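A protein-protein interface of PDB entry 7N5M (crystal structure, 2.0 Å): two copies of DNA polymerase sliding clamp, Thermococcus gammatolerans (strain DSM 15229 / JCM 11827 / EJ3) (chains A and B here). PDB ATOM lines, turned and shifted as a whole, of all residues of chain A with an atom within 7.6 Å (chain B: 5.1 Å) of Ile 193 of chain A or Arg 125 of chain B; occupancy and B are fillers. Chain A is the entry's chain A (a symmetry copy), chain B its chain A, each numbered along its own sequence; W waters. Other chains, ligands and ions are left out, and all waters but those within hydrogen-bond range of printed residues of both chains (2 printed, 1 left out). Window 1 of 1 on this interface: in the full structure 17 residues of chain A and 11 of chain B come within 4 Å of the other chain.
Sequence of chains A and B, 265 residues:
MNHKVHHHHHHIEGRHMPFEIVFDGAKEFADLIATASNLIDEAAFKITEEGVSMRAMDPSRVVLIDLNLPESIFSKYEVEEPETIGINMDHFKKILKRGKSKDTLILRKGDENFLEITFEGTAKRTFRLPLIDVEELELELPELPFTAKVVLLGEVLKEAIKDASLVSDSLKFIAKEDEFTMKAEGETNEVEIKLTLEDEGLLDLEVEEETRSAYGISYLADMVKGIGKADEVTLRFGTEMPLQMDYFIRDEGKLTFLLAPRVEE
NH1 of Arg 98 of chain B is in salt-bridge range of OD1 of Asp 163 of chain A, 3.2 Å away. The backbone NH (N) of Lys 194 of chain A is in hydrogen-bond range of the backbone carbonyl oxygen (O) of Lys 124 of chain B (2.8 Å). The guanidinium group of Arg 125 of chain B is in salt-bridge range of the side-chain carboxylate of Glu 159 of chain A, 3.8 Å away. The guanidinium group (NH1) of Arg 125 of chain B is in salt-bridge range of the side-chain carboxylate (OD2) of Asp 163 of chain A (3.0 Å). N of Thr 126 of chain B is in hydrogen-bond range of O of Glu 192 of chain A (2.8 Å).
The guanidinium group of Arg 125 of chain B lies within hydrogen-bond range of the backbone carbonyl oxygen of Arg 98 of chain B (2.8 Å). OG1 of Thr 126 of chain B lies within hydrogen-bond range of OG1 of Thr 118 of chain B, 3.1 Å away. N of Leu 195 of chain A lies within hydrogen-bond range of O of Phe 180 of chain A (2.8 Å). The side-chain hydroxyl (OG1) of Thr 181 of chain A is in hydrogen-bond range of the side-chain amino group (NZ) of Lys 194 of chain A. NZ of Lys 183 of chain A lies within salt-bridge range of OE1 of Glu 192 of chain A (3.9 Å). The side-chain carboxylate (OE2) of Glu 192 of chain A lies within salt-bridge range of the side-chain amino group (NZ) of Lys 194 of chain A (2.6 Å).
Glu 159 of chain A touches Arg 98 of chain B. CE of Lys 100 of chain B touches OE1 of Glu 159 of chain A (3.4 Å). NH1 of Arg 98 of chain B touches CG of Lys 162 of chain A (3.7 Å). CG of Asp 163 of chain A touches CZ of Phe 127 of chain B, at 3.5 Å. Glu 190 of chain A touches Thr 126 of chain B (O to O, 3.8 Å). CA of Phe 127 of chain B touches O of Glu 190 of chain A, 3.3 Å away. O of Thr 126 of chain B touches CA of Val 191 of chain A, 3.3 Å away. Val 191 of chain A touches Phe 127 of chain B. O of Glu 192 of chain A touches CA of Arg 125 of chain B (3.3 Å). CG of Arg 125 of chain B touches CG2 of Ile 193 of chain A (3.99 Å).
Printed residues of chain B within 4 Å of Ile 193 of chain A: Lys 124 and Arg 125. Of the printed residues of chain A, Arg 125 of chain B touches Glu 159 (3.7 Å), Asp 163 (3.0 Å), Glu 192 (3.3 Å) and Ile 193 (3.99 Å). Of the printed residues of chain B, Glu 192 of chain A touches Lys 124 (3.7 Å), Arg 125 (3.3 Å) and Thr 126 (2.8 Å). Of the printed residues of chain B, Val 191 of chain A touches Thr 126 and Phe 127. Of the printed residues of chain B, Glu 159 of chain A touches Arg 98, Lys 100 and Arg 125. Phe 180 of chain A touches none of the printed residues of chain B. The nearest printed residue of chain B that does not touch Asp 163 of chain A is Phe 119 of chain B (5.9 Å).
Along chain B the printed residues that touch a printed residue of chain A span positions 98 to 127. Printed residues of chain A that touch a printed residue of chain B: Glu 159, Lys 162, Asp 163, Glu 190, Val 191, Glu 192, Ile 193, Lys 194 and Leu 195. Hydrophobic or aromatic side chains of chain A within 4 Å of the printed part of chain B: Val 191, Ile 193 and Leu 195.
No position is printed for both chains.
Water W1 lies within hydrogen-bond range of O of Thr 126 of chain B (2.9 Å) and OE2 of Glu 190 of chain A (3.3 Å). Water W2 lies within hydrogen-bond range of OG1 of Thr 126 of chain B (3.0 Å), O of Glu 192 of chain A (3.2 Å) and O of Lys 124 of chain B (3.3 Å).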
ATOM      1  N   LEU A 152      -4.853  34.797   7.481  1.00  0.00           N
ATOM      2  CA  LEU A 152      -6.179  34.692   6.892  1.00  0.00           C
ATOM      3  C   LEU A 152      -7.187  34.270   7.938  1.00  0.00           C
ATOM      4  O   LEU A 152      -6.852  33.753   9.007  1.00  0.00           O
ATOM      5  CB  LEU A 152      -6.244  33.727   5.691  1.00  0.00           C
ATOM      6  CG  LEU A 152      -5.733  32.286   5.672  1.00  0.00           C
ATOM      7  CD1 LEU A 152      -6.339  31.441   6.747  1.00  0.00           C
ATOM      8  CD2 LEU A 152      -6.022  31.664   4.306  1.00  0.00           C
ATOM      9  N   GLU A 155     -12.226  30.761   8.663  1.00  0.00           N
ATOM     10  CA  GLU A 155     -13.281  30.226   7.813  1.00  0.00           C
ATOM     11  C   GLU A 155     -12.798  29.995   6.389  1.00  0.00           C
ATOM     12  O   GLU A 155     -13.210  29.024   5.746  1.00  0.00           O
ATOM     13  CB  GLU A 155     -14.487  31.166   7.822  1.00  0.00           C
ATOM     14  CG  GLU A 155     -14.212  32.514   7.208  1.00  0.00           C
ATOM     15  CD  GLU A 155     -14.976  32.716   5.919  1.00  0.00           C
ATOM     16  OE1 GLU A 155     -15.288  31.716   5.242  1.00  0.00           O
ATOM     17  OE2 GLU A 155     -15.275  33.874   5.593  1.00  0.00           O
ATOM     18  N   VAL A 156     -11.908  30.853   5.888  1.00  0.00           N
ATOM     19  CA  VAL A 156     -11.380  30.674   4.541  1.00  0.00           C
ATOM     20  C   VAL A 156     -10.487  29.447   4.497  1.00  0.00           C
ATOM     21  O   VAL A 156     -10.595  28.609   3.598  1.00  0.00           O
ATOM     22  CB  VAL A 156     -10.629  31.930   4.063  1.00  0.00           C
ATOM     23  CG1 VAL A 156      -9.776  31.586   2.849  1.00  0.00           C
ATOM     24  CG2 VAL A 156     -11.609  33.050   3.723  1.00  0.00           C
ATOM     25  N   LEU A 157      -9.600  29.323   5.487  1.00  0.00           N
ATOM     26  CA  LEU A 157      -8.728  28.161   5.579  1.00  0.00           C
ATOM     27  C   LEU A 157      -9.538  26.877   5.726  1.00  0.00           C
ATOM     28  O   LEU A 157      -9.322  25.908   4.990  1.00  0.00           O
ATOM     29  CB  LEU A 157      -7.774  28.346   6.760  1.00  0.00           C
ATOM     30  CG  LEU A 157      -6.749  27.265   7.047  1.00  0.00           C
ATOM     31  CD1 LEU A 157      -5.838  27.088   5.842  1.00  0.00           C
ATOM     32  CD2 LEU A 157      -5.945  27.635   8.313  1.00  0.00           C
ATOM     33  N   GLU A 159     -12.725  26.263   5.020  1.00  0.00           N
ATOM     34  CA  GLU A 159     -13.536  25.930   3.845  1.00  0.00           C
ATOM     35  C   GLU A 159     -12.673  25.466   2.685  1.00  0.00           C
ATOM     36  O   GLU A 159     -13.071  24.555   1.948  1.00  0.00           O
ATOM     37  CB  GLU A 159     -14.425  27.116   3.419  1.00  0.00           C
ATOM     38  CG  GLU A 159     -13.770  28.162   2.513  1.00  0.00           C
ATOM     39  CD  GLU A 159     -14.496  29.521   2.540  1.00  0.00           C
ATOM     40  OE1 GLU A 159     -15.708  29.578   2.856  1.00  0.00           O
ATOM     41  OE2 GLU A 159     -13.841  30.537   2.232  1.00  0.00           O
ATOM     42  N   ALA A 160     -11.470  26.036   2.540  1.00  0.00           N
ATOM     43  CA  ALA A 160     -10.595  25.667   1.435  1.00  0.00           C
ATOM     44  C   ALA A 160     -10.146  24.225   1.550  1.00  0.00           C
ATOM     45  O   ALA A 160     -10.038  23.513   0.550  1.00  0.00           O
ATOM     46  CB  ALA A 160      -9.376  26.595   1.406  1.00  0.00           C
ATOM     47  N   ILE A 161      -9.851  23.793   2.772  1.00  0.00           N
ATOM     48  CA  ILE A 161      -9.434  22.423   2.993  1.00  0.00           C
ATOM     49  C   ILE A 161     -10.599  21.471   2.731  1.00  0.00           C
ATOM     50  O   ILE A 161     -10.435  20.427   2.092  1.00  0.00           O
ATOM     51  CB  ILE A 161      -8.852  22.308   4.422  1.00  0.00           C
ATOM     52  CG1 ILE A 161      -7.497  23.046   4.482  1.00  0.00           C
ATOM     53  CG2 ILE A 161      -8.726  20.833   4.858  1.00  0.00           C
ATOM     54  CD1 ILE A 161      -7.092  23.497   5.900  1.00  0.00           C
ATOM     55  N   LYS A 162     -11.801  21.836   3.171  1.00  0.00           N
ATOM     56  CA  LYS A 162     -12.982  21.035   2.847  1.00  0.00           C
ATOM     57  C   LYS A 162     -13.244  21.021   1.340  1.00  0.00           C
ATOM     58  O   LYS A 162     -13.484  19.960   0.750  1.00  0.00           O
ATOM     59  CB  LYS A 162     -14.191  21.577   3.609  1.00  0.00           C
ATOM     60  CG  LYS A 162     -15.383  20.653   3.677  1.00  0.00           C
ATOM     61  CD  LYS A 162     -16.041  20.733   5.051  1.00  0.00           C
ATOM     62  CE  LYS A 162     -15.891  22.121   5.666  1.00  0.00           C
ATOM     63  NZ  LYS A 162     -16.008  22.110   7.161  1.00  0.00           N
ATOM     64  N   ASP A 163     -13.186  22.191   0.697  1.00  0.00           N
ATOM     65  CA  ASP A 163     -13.317  22.260  -0.762  1.00  0.00           C
ATOM     66  C   ASP A 163     -12.348  21.319  -1.452  1.00  0.00           C
ATOM     67  O   ASP A 163     -12.718  20.588  -2.375  1.00  0.00           O
ATOM     68  CB  ASP A 163     -13.066  23.690  -1.257  1.00  0.00           C
ATOM     69  CG  ASP A 163     -14.079  24.670  -0.735  1.00  0.00           C
ATOM     70  OD1 ASP A 163     -15.105  24.216  -0.196  1.00  0.00           O
ATOM     71  OD2 ASP A 163     -13.838  25.892  -0.833  1.00  0.00           O
ATOM     72  N   ALA A 164     -11.080  21.353  -1.035  1.00  0.00           N
ATOM     73  CA  ALA A 164     -10.053  20.583  -1.719  1.00  0.00           C
ATOM     74  C   ALA A 164     -10.265  19.095  -1.528  1.00  0.00           C
ATOM     75  O   ALA A 164      -9.966  18.303  -2.431  1.00  0.00           O
ATOM     76  CB  ALA A 164      -8.671  20.996  -1.208  1.00  0.00           C
ATOM     77  N   LEU A 171      -3.174  19.440  -1.049  1.00  0.00           N
ATOM     78  CA  LEU A 171      -3.507  20.835  -1.288  1.00  0.00           C
ATOM     79  C   LEU A 171      -2.222  21.602  -1.553  1.00  0.00           C
ATOM     80  O   LEU A 171      -1.354  21.686  -0.674  1.00  0.00           O
ATOM     81  CB  LEU A 171      -4.253  21.430  -0.088  1.00  0.00           C
ATOM     82  CG  LEU A 171      -4.853  22.828  -0.276  1.00  0.00           C
ATOM     83  CD1 LEU A 171      -5.697  22.898  -1.547  1.00  0.00           C
ATOM     84  CD2 LEU A 171      -5.678  23.196   0.954  1.00  0.00           C
ATOM     85  N   LYS A 172      -2.118  22.192  -2.742  1.00  0.00           N
ATOM     86  CA  LYS A 172      -0.972  23.020  -3.102  1.00  0.00           C
ATOM     87  C   LYS A 172      -1.179  24.454  -2.613  1.00  0.00           C
ATOM     88  O   LYS A 172      -2.237  25.051  -2.839  1.00  0.00           O
ATOM     89  CB  LYS A 172      -0.752  22.995  -4.617  1.00  0.00           C
ATOM     90  CG  LYS A 172      -0.543  21.593  -5.184  1.00  0.00           C
ATOM     91  CD  LYS A 172      -1.198  21.437  -6.556  1.00  0.00           C
ATOM     92  CE  LYS A 172      -0.297  22.001  -7.643  1.00  0.00           C
ATOM     93  NZ  LYS A 172       0.701  21.004  -8.132  1.00  0.00           N
ATOM     94  N   ILE A 174       0.238  28.273  -2.960  1.00  0.00           N
ATOM     95  CA  ILE A 174       0.990  29.119  -3.891  1.00  0.00           C
ATOM     96  C   ILE A 174       0.897  30.565  -3.427  1.00  0.00           C
ATOM     97  O   ILE A 174      -0.184  31.167  -3.466  1.00  0.00           O
ATOM     98  CB  ILE A 174       0.489  28.999  -5.336  1.00  0.00           C
ATOM     99  CG1 ILE A 174       0.605  27.556  -5.841  1.00  0.00           C
ATOM    100  CG2 ILE A 174       1.304  29.926  -6.236  1.00  0.00           C
ATOM    101  CD1 ILE A 174      -0.362  27.229  -6.964  1.00  0.00           C
ATOM    102  N   PHE A 180      -2.470  34.829  -2.791  1.00  0.00           N
ATOM    103  CA  PHE A 180      -2.251  33.531  -2.179  1.00  0.00           C
ATOM    104  C   PHE A 180      -3.284  32.590  -2.769  1.00  0.00           C
ATOM    105  O   PHE A 180      -4.480  32.897  -2.750  1.00  0.00           O
ATOM    106  CB  PHE A 180      -2.380  33.618  -0.651  1.00  0.00           C
ATOM    107  CG  PHE A 180      -2.370  32.286   0.044  1.00  0.00           C
ATOM    108  CD1 PHE A 180      -1.318  31.395  -0.140  1.00  0.00           C
ATOM    109  CD2 PHE A 180      -3.408  31.924   0.881  1.00  0.00           C
ATOM    110  CE1 PHE A 180      -1.305  30.166   0.502  1.00  0.00           C
ATOM    111  CE2 PHE A 180      -3.401  30.697   1.515  1.00  0.00           C
ATOM    112  CZ  PHE A 180      -2.341  29.817   1.323  1.00  0.00           C
ATOM    113  N   THR A 181      -2.827  31.466  -3.318  1.00  0.00           N
ATOM    114  CA  THR A 181      -3.706  30.501  -3.962  1.00  0.00           C
ATOM    115  C   THR A 181      -3.530  29.136  -3.308  1.00  0.00           C
ATOM    116  O   THR A 181      -2.400  28.700  -3.073  1.00  0.00           O
ATOM    117  CB  THR A 181      -3.425  30.418  -5.477  1.00  0.00           C
ATOM    118  OG1 THR A 181      -3.813  31.651  -6.110  1.00  0.00           O
ATOM    119  CG2 THR A 181      -4.220  29.284  -6.105  1.00  0.00           C
ATOM    120  N   MET A 182      -4.648  28.485  -2.984  1.00  0.00           N
ATOM    121  CA  MET A 182      -4.653  27.085  -2.577  1.00  0.00           C
ATOM    122  C   MET A 182      -5.410  26.298  -3.632  1.00  0.00           C
ATOM    123  O   MET A 182      -6.575  26.596  -3.912  1.00  0.00           O
ATOM    124  CB  MET A 182      -5.282  26.886  -1.199  1.00  0.00           C
ATOM    125  CG  MET A 182      -4.558  27.621  -0.074  1.00  0.00           C
ATOM    126  SD  MET A 182      -5.469  27.554   1.485  1.00  0.00           S
ATOM    127  CE  MET A 182      -6.615  28.905   1.276  1.00  0.00           C
ATOM    128  N   LYS A 183      -4.749  25.293  -4.209  1.00  0.00           N
ATOM    129  CA  LYS A 183      -5.279  24.612  -5.379  1.00  0.00           C
ATOM    130  C   LYS A 183      -5.150  23.106  -5.209  1.00  0.00           C
ATOM    131  O   LYS A 183      -4.106  22.602  -4.782  1.00  0.00           O
ATOM    132  CB  LYS A 183      -4.553  25.096  -6.649  1.00  0.00           C
ATOM    133  CG  LYS A 183      -4.511  24.087  -7.785  1.00  0.00           C
ATOM    134  CD  LYS A 183      -3.670  24.601  -8.962  1.00  0.00           C
ATOM    135  CE  LYS A 183      -3.678  26.132  -9.042  1.00  0.00           C
ATOM    136  NZ  LYS A 183      -3.136  26.646 -10.340  1.00  0.00           N
ATOM    137  N   ALA A 184      -6.222  22.393  -5.539  1.00  0.00           N
ATOM    138  CA  ALA A 184      -6.249  20.942  -5.520  1.00  0.00           C
ATOM    139  C   ALA A 184      -6.772  20.434  -6.857  1.00  0.00           C
ATOM    140  O   ALA A 184      -7.659  21.048  -7.463  1.00  0.00           O
ATOM    141  CB  ALA A 184      -7.121  20.429  -4.394  1.00  0.00           C
ATOM    142  N   GLU A 190     -11.639  19.849 -10.029  1.00  0.00           N
ATOM    143  CA  GLU A 190     -10.518  20.729  -9.718  1.00  0.00           C
ATOM    144  C   GLU A 190     -11.050  21.904  -8.911  1.00  0.00           C
ATOM    145  O   GLU A 190     -12.171  22.363  -9.134  1.00  0.00           O
ATOM    146  CB  GLU A 190      -9.806  21.236 -10.973  1.00  0.00           C
ATOM    147  CG  GLU A 190      -8.468  21.887 -10.667  1.00  0.00           C
ATOM    148  CD  GLU A 190      -8.187  23.120 -11.510  1.00  0.00           C
ATOM    149  OE1 GLU A 190      -8.215  23.012 -12.758  1.00  0.00           O
ATOM    150  OE2 GLU A 190      -7.927  24.195 -10.912  1.00  0.00           O
ATOM    151  N   VAL A 191     -10.253  22.375  -7.959  1.00  0.00           N
ATOM    152  CA  VAL A 191     -10.676  23.483  -7.111  1.00  0.00           C
ATOM    153  C   VAL A 191      -9.502  24.421  -6.896  1.00  0.00           C
ATOM    154  O   VAL A 191      -8.359  23.981  -6.733  1.00  0.00           O
ATOM    155  CB  VAL A 191     -11.257  23.011  -5.760  1.00  0.00           C
ATOM    156  CG1 VAL A 191     -10.202  22.339  -4.925  1.00  0.00           C
ATOM    157  CG2 VAL A 191     -11.830  24.190  -5.000  1.00  0.00           C
ATOM    158  N   GLU A 192      -9.799  25.718  -6.905  1.00  0.00           N
ATOM    159  CA  GLU A 192      -8.829  26.770  -6.658  1.00  0.00           C
ATOM    160  C   GLU A 192      -9.454  27.791  -5.717  1.00  0.00           C
ATOM    161  O   GLU A 192     -10.567  28.271  -5.965  1.00  0.00           O
ATOM    162  CB  GLU A 192      -8.425  27.418  -7.977  1.00  0.00           C
ATOM    163  CG  GLU A 192      -7.244  28.314  -7.929  1.00  0.00           C
ATOM    164  CD  GLU A 192      -6.730  28.583  -9.332  1.00  0.00           C
ATOM    165  OE1 GLU A 192      -6.855  27.678 -10.192  1.00  0.00           O
ATOM    166  OE2 GLU A 192      -6.235  29.697  -9.578  1.00  0.00           O
ATOM    167  N   ILE A 193      -8.756  28.101  -4.624  1.00  0.00           N
ATOM    168  CA  ILE A 193      -9.174  29.146  -3.692  1.00  0.00           C
ATOM    169  C   ILE A 193      -8.130  30.245  -3.772  1.00  0.00           C
ATOM    170  O   ILE A 193      -6.933  29.987  -3.569  1.00  0.00           O
ATOM    171  CB  ILE A 193      -9.332  28.629  -2.251  1.00  0.00           C
ATOM    172  CG1 ILE A 193     -10.332  27.469  -2.181  1.00  0.00           C
ATOM    173  CG2 ILE A 193      -9.759  29.767  -1.303  1.00  0.00           C
ATOM    174  CD1 ILE A 193      -9.718  26.037  -2.405  1.00  0.00           C
ATOM    175  N   LYS A 194      -8.574  31.458  -4.079  1.00  0.00           N
ATOM    176  CA  LYS A 194      -7.671  32.566  -4.348  1.00  0.00           C
ATOM    177  C   LYS A 194      -7.987  33.723  -3.416  1.00  0.00           C
ATOM    178  O   LYS A 194      -9.158  34.067  -3.201  1.00  0.00           O
ATOM    179  CB  LYS A 194      -7.755  33.021  -5.817  1.00  0.00           C
ATOM    180  CG  LYS A 194      -6.603  33.940  -6.240  1.00  0.00           C
ATOM    181  CD  LYS A 194      -6.477  34.045  -7.763  1.00  0.00           C
ATOM    182  CE  LYS A 194      -6.614  32.684  -8.456  1.00  0.00           C
ATOM    183  NZ  LYS A 194      -5.360  31.855  -8.408  1.00  0.00           N
ATOM    184  N   LEU A 195      -6.931  34.301  -2.841  1.00  0.00           N
ATOM    185  CA  LEU A 195      -7.051  35.456  -1.967  1.00  0.00           C
ATOM    186  C   LEU A 195      -6.111  36.558  -2.440  1.00  0.00           C
ATOM    187  O   LEU A 195      -4.970  36.292  -2.838  1.00  0.00           O
ATOM    188  CB  LEU A 195      -6.724  35.089  -0.516  1.00  0.00           C
ATOM    189  CG  LEU A 195      -7.776  34.290   0.257  1.00  0.00           C
ATOM    190  CD1 LEU A 195      -7.120  33.586   1.435  1.00  0.00           C
ATOM    191  CD2 LEU A 195      -8.887  35.193   0.741  1.00  0.00           C
ATOM    192  N   ARG B  98     -20.970  23.786  -0.928  1.00  0.00           N
ATOM    193  CA  ARG B  98     -19.839  24.543  -0.399  1.00  0.00           C
ATOM    194  C   ARG B  98     -20.084  26.055  -0.397  1.00  0.00           C
ATOM    195  O   ARG B  98     -19.356  26.788   0.278  1.00  0.00           O
ATOM    196  CB  ARG B  98     -18.597  24.199  -1.210  1.00  0.00           C
ATOM    197  CG  ARG B  98     -18.208  22.687  -1.149  1.00  0.00           C
ATOM    198  CD  ARG B  98     -17.573  22.267   0.177  1.00  0.00           C
ATOM    199  NE  ARG B  98     -18.435  22.422   1.344  1.00  0.00           N
ATOM    200  CZ  ARG B  98     -18.099  23.144   2.403  1.00  0.00           C
ATOM    201  NH1 ARG B  98     -16.932  23.780   2.408  1.00  0.00           N
ATOM    202  NH2 ARG B  98     -18.926  23.257   3.426  1.00  0.00           N
ATOM    203  N   GLY B  99     -21.094  26.539  -1.114  1.00  0.00           N
ATOM    204  CA  GLY B  99     -21.345  27.979  -1.150  1.00  0.00           C
ATOM    205  C   GLY B  99     -21.899  28.522   0.163  1.00  0.00           C
ATOM    206  O   GLY B  99     -22.696  27.880   0.845  1.00  0.00           O
ATOM    207  N   LYS B 100     -21.488  29.738   0.508  1.00  0.00           N
ATOM    208  CA  LYS B 100     -21.968  30.348   1.741  1.00  0.00           C
ATOM    209  C   LYS B 100     -23.162  31.242   1.450  1.00  0.00           C
ATOM    210  O   LYS B 100     -23.426  31.615   0.301  1.00  0.00           O
ATOM    211  CB  LYS B 100     -20.856  31.143   2.433  1.00  0.00           C
ATOM    212  CG  LYS B 100     -19.592  30.323   2.642  1.00  0.00           C
ATOM    213  CD  LYS B 100     -19.930  28.982   3.284  1.00  0.00           C
ATOM    214  CE  LYS B 100     -18.705  28.115   3.514  1.00  0.00           C
ATOM    215  NZ  LYS B 100     -19.107  26.841   4.167  1.00  0.00           N
ATOM    216  N   ASP B 103     -22.139  34.357  -0.257  1.00  0.00           N
ATOM    217  CA  ASP B 103     -21.366  34.199  -1.476  1.00  0.00           C
ATOM    218  C   ASP B 103     -22.189  34.631  -2.683  1.00  0.00           C
ATOM    219  O   ASP B 103     -23.406  34.433  -2.729  1.00  0.00           O
ATOM    220  CB  ASP B 103     -20.948  32.729  -1.651  1.00  0.00           C
ATOM    221  CG  ASP B 103     -19.726  32.362  -0.834  1.00  0.00           C
ATOM    222  OD1 ASP B 103     -18.875  33.242  -0.592  1.00  0.00           O
ATOM    223  OD2 ASP B 103     -19.618  31.188  -0.444  1.00  0.00           O
ATOM    224  N   ILE B 117     -17.690  26.833 -11.633  1.00  0.00           N
ATOM    225  CA  ILE B 117     -18.570  27.257 -10.553  1.00  0.00           C
ATOM    226  C   ILE B 117     -17.726  28.035  -9.561  1.00  0.00           C
ATOM    227  O   ILE B 117     -16.819  27.471  -8.934  1.00  0.00           O
ATOM    228  CB  ILE B 117     -19.264  26.068  -9.875  1.00  0.00           C
ATOM    229  CG1 ILE B 117     -20.134  25.303 -10.881  1.00  0.00           C
ATOM    230  CG2 ILE B 117     -20.097  26.572  -8.693  1.00  0.00           C
ATOM    231  CD1 ILE B 117     -20.474  23.874 -10.486  1.00  0.00           C
ATOM    232  N   THR B 118     -18.029  29.322  -9.416  1.00  0.00           N
ATOM    233  CA  THR B 118     -17.251  30.221  -8.577  1.00  0.00           C
ATOM    234  C   THR B 118     -18.124  30.740  -7.450  1.00  0.00           C
ATOM    235  O   THR B 118     -19.249  31.201  -7.692  1.00  0.00           O
ATOM    236  CB  THR B 118     -16.684  31.386  -9.395  1.00  0.00           C
ATOM    237  OG1 THR B 118     -15.784  30.865 -10.375  1.00  0.00           O
ATOM    238  CG2 THR B 118     -15.942  32.400  -8.494  1.00  0.00           C
ATOM    239  N   PHE B 119     -17.606  30.659  -6.221  1.00  0.00           N
ATOM    240  CA  PHE B 119     -18.173  31.369  -5.082  1.00  0.00           C
ATOM    241  C   PHE B 119     -17.309  32.588  -4.792  1.00  0.00           C
ATOM    242  O   PHE B 119     -16.091  32.459  -4.625  1.00  0.00           O
ATOM    243  CB  PHE B 119     -18.254  30.470  -3.847  1.00  0.00           C
ATOM    244  CG  PHE B 119     -18.962  29.180  -4.095  1.00  0.00           C
ATOM    245  CD1 PHE B 119     -20.317  29.168  -4.380  1.00  0.00           C
ATOM    246  CD2 PHE B 119     -18.279  27.977  -4.047  1.00  0.00           C
ATOM    247  CE1 PHE B 119     -20.985  27.982  -4.627  1.00  0.00           C
ATOM    248  CE2 PHE B 119     -18.939  26.763  -4.295  1.00  0.00           C
ATOM    249  CZ  PHE B 119     -20.311  26.770  -4.599  1.00  0.00           C
ATOM    250  N   ALA B 123     -13.437  35.071  -0.035  1.00  0.00           N
ATOM    251  CA  ALA B 123     -12.421  34.554  -0.940  1.00  0.00           C
ATOM    252  C   ALA B 123     -13.111  34.186  -2.244  1.00  0.00           C
ATOM    253  O   ALA B 123     -14.338  34.086  -2.303  1.00  0.00           O
ATOM    254  CB  ALA B 123     -11.708  33.327  -0.355  1.00  0.00           C
ATOM    255  N   LYS B 124     -12.311  33.982  -3.292  1.00  0.00           N
ATOM    256  CA  LYS B 124     -12.801  33.474  -4.566  1.00  0.00           C
ATOM    257  C   LYS B 124     -12.466  31.986  -4.656  1.00  0.00           C
ATOM    258  O   LYS B 124     -11.292  31.604  -4.600  1.00  0.00           O
ATOM    259  CB  LYS B 124     -12.187  34.233  -5.744  1.00  0.00           C
ATOM    260  CG  LYS B 124     -12.663  33.724  -7.114  1.00  0.00           C
ATOM    261  CD  LYS B 124     -11.741  34.201  -8.238  1.00  0.00           C
ATOM    262  CE  LYS B 124     -12.431  34.170  -9.593  1.00  0.00           C
ATOM    263  NZ  LYS B 124     -11.506  34.630 -10.666  1.00  0.00           N
ATOM    264  N   ARG B 125     -13.495  31.148  -4.776  1.00  0.00           N
ATOM    265  CA  ARG B 125     -13.304  29.705  -4.847  1.00  0.00           C
ATOM    266  C   ARG B 125     -13.950  29.186  -6.121  1.00  0.00           C
ATOM    267  O   ARG B 125     -15.154  29.370  -6.325  1.00  0.00           O
ATOM    268  CB  ARG B 125     -13.899  29.008  -3.621  1.00  0.00           C
ATOM    269  CG  ARG B 125     -13.623  29.737  -2.298  1.00  0.00           C
ATOM    270  CD  ARG B 125     -14.298  29.025  -1.146  1.00  0.00           C
ATOM    271  NE  ARG B 125     -15.677  29.449  -0.972  1.00  0.00           N
ATOM    272  CZ  ARG B 125     -16.658  28.630  -0.623  1.00  0.00           C
ATOM    273  NH1 ARG B 125     -16.398  27.351  -0.446  1.00  0.00           N
ATOM    274  NH2 ARG B 125     -17.895  29.082  -0.463  1.00  0.00           N
ATOM    275  N   THR B 126     -13.166  28.498  -6.947  1.00  0.00           N
ATOM    276  CA  THR B 126     -13.584  28.087  -8.282  1.00  0.00           C
ATOM    277  C   THR B 126     -13.460  26.575  -8.421  1.00  0.00           C
ATOM    278  O   THR B 126     -12.375  26.016  -8.240  1.00  0.00           O
ATOM    279  CB  THR B 126     -12.739  28.819  -9.333  1.00  0.00           C
ATOM    280  OG1 THR B 126     -12.963  30.225  -9.200  1.00  0.00           O
ATOM    281  CG2 THR B 126     -13.085  28.366 -10.742  1.00  0.00           C
ATOM    282  N   PHE B 127     -14.580  25.918  -8.708  1.00  0.00           N
ATOM    283  CA  PHE B 127     -14.639  24.499  -9.008  1.00  0.00           C
ATOM    284  C   PHE B 127     -14.892  24.311 -10.496  1.00  0.00           C
ATOM    285  O   PHE B 127     -15.587  25.106 -11.128  1.00  0.00           O
ATOM    286  CB  PHE B 127     -15.764  23.802  -8.238  1.00  0.00           C
ATOM    287  CG  PHE B 127     -15.644  23.886  -6.727  1.00  0.00           C
ATOM    288  CD1 PHE B 127     -15.936  25.064  -6.059  1.00  0.00           C
ATOM    289  CD2 PHE B 127     -15.287  22.769  -5.980  1.00  0.00           C
ATOM    290  CE1 PHE B 127     -15.851  25.141  -4.659  1.00  0.00           C
ATOM    291  CE2 PHE B 127     -15.197  22.842  -4.577  1.00  0.00           C
ATOM    292  CZ  PHE B 127     -15.492  24.031  -3.923  1.00  0.00           C
HETATM  293  O   HOH W   1     -10.868  25.716 -10.700  1.00  0.00           O
HETATM  294  O   HOH W   2     -10.482  30.966  -7.768  1.00  0.00           O
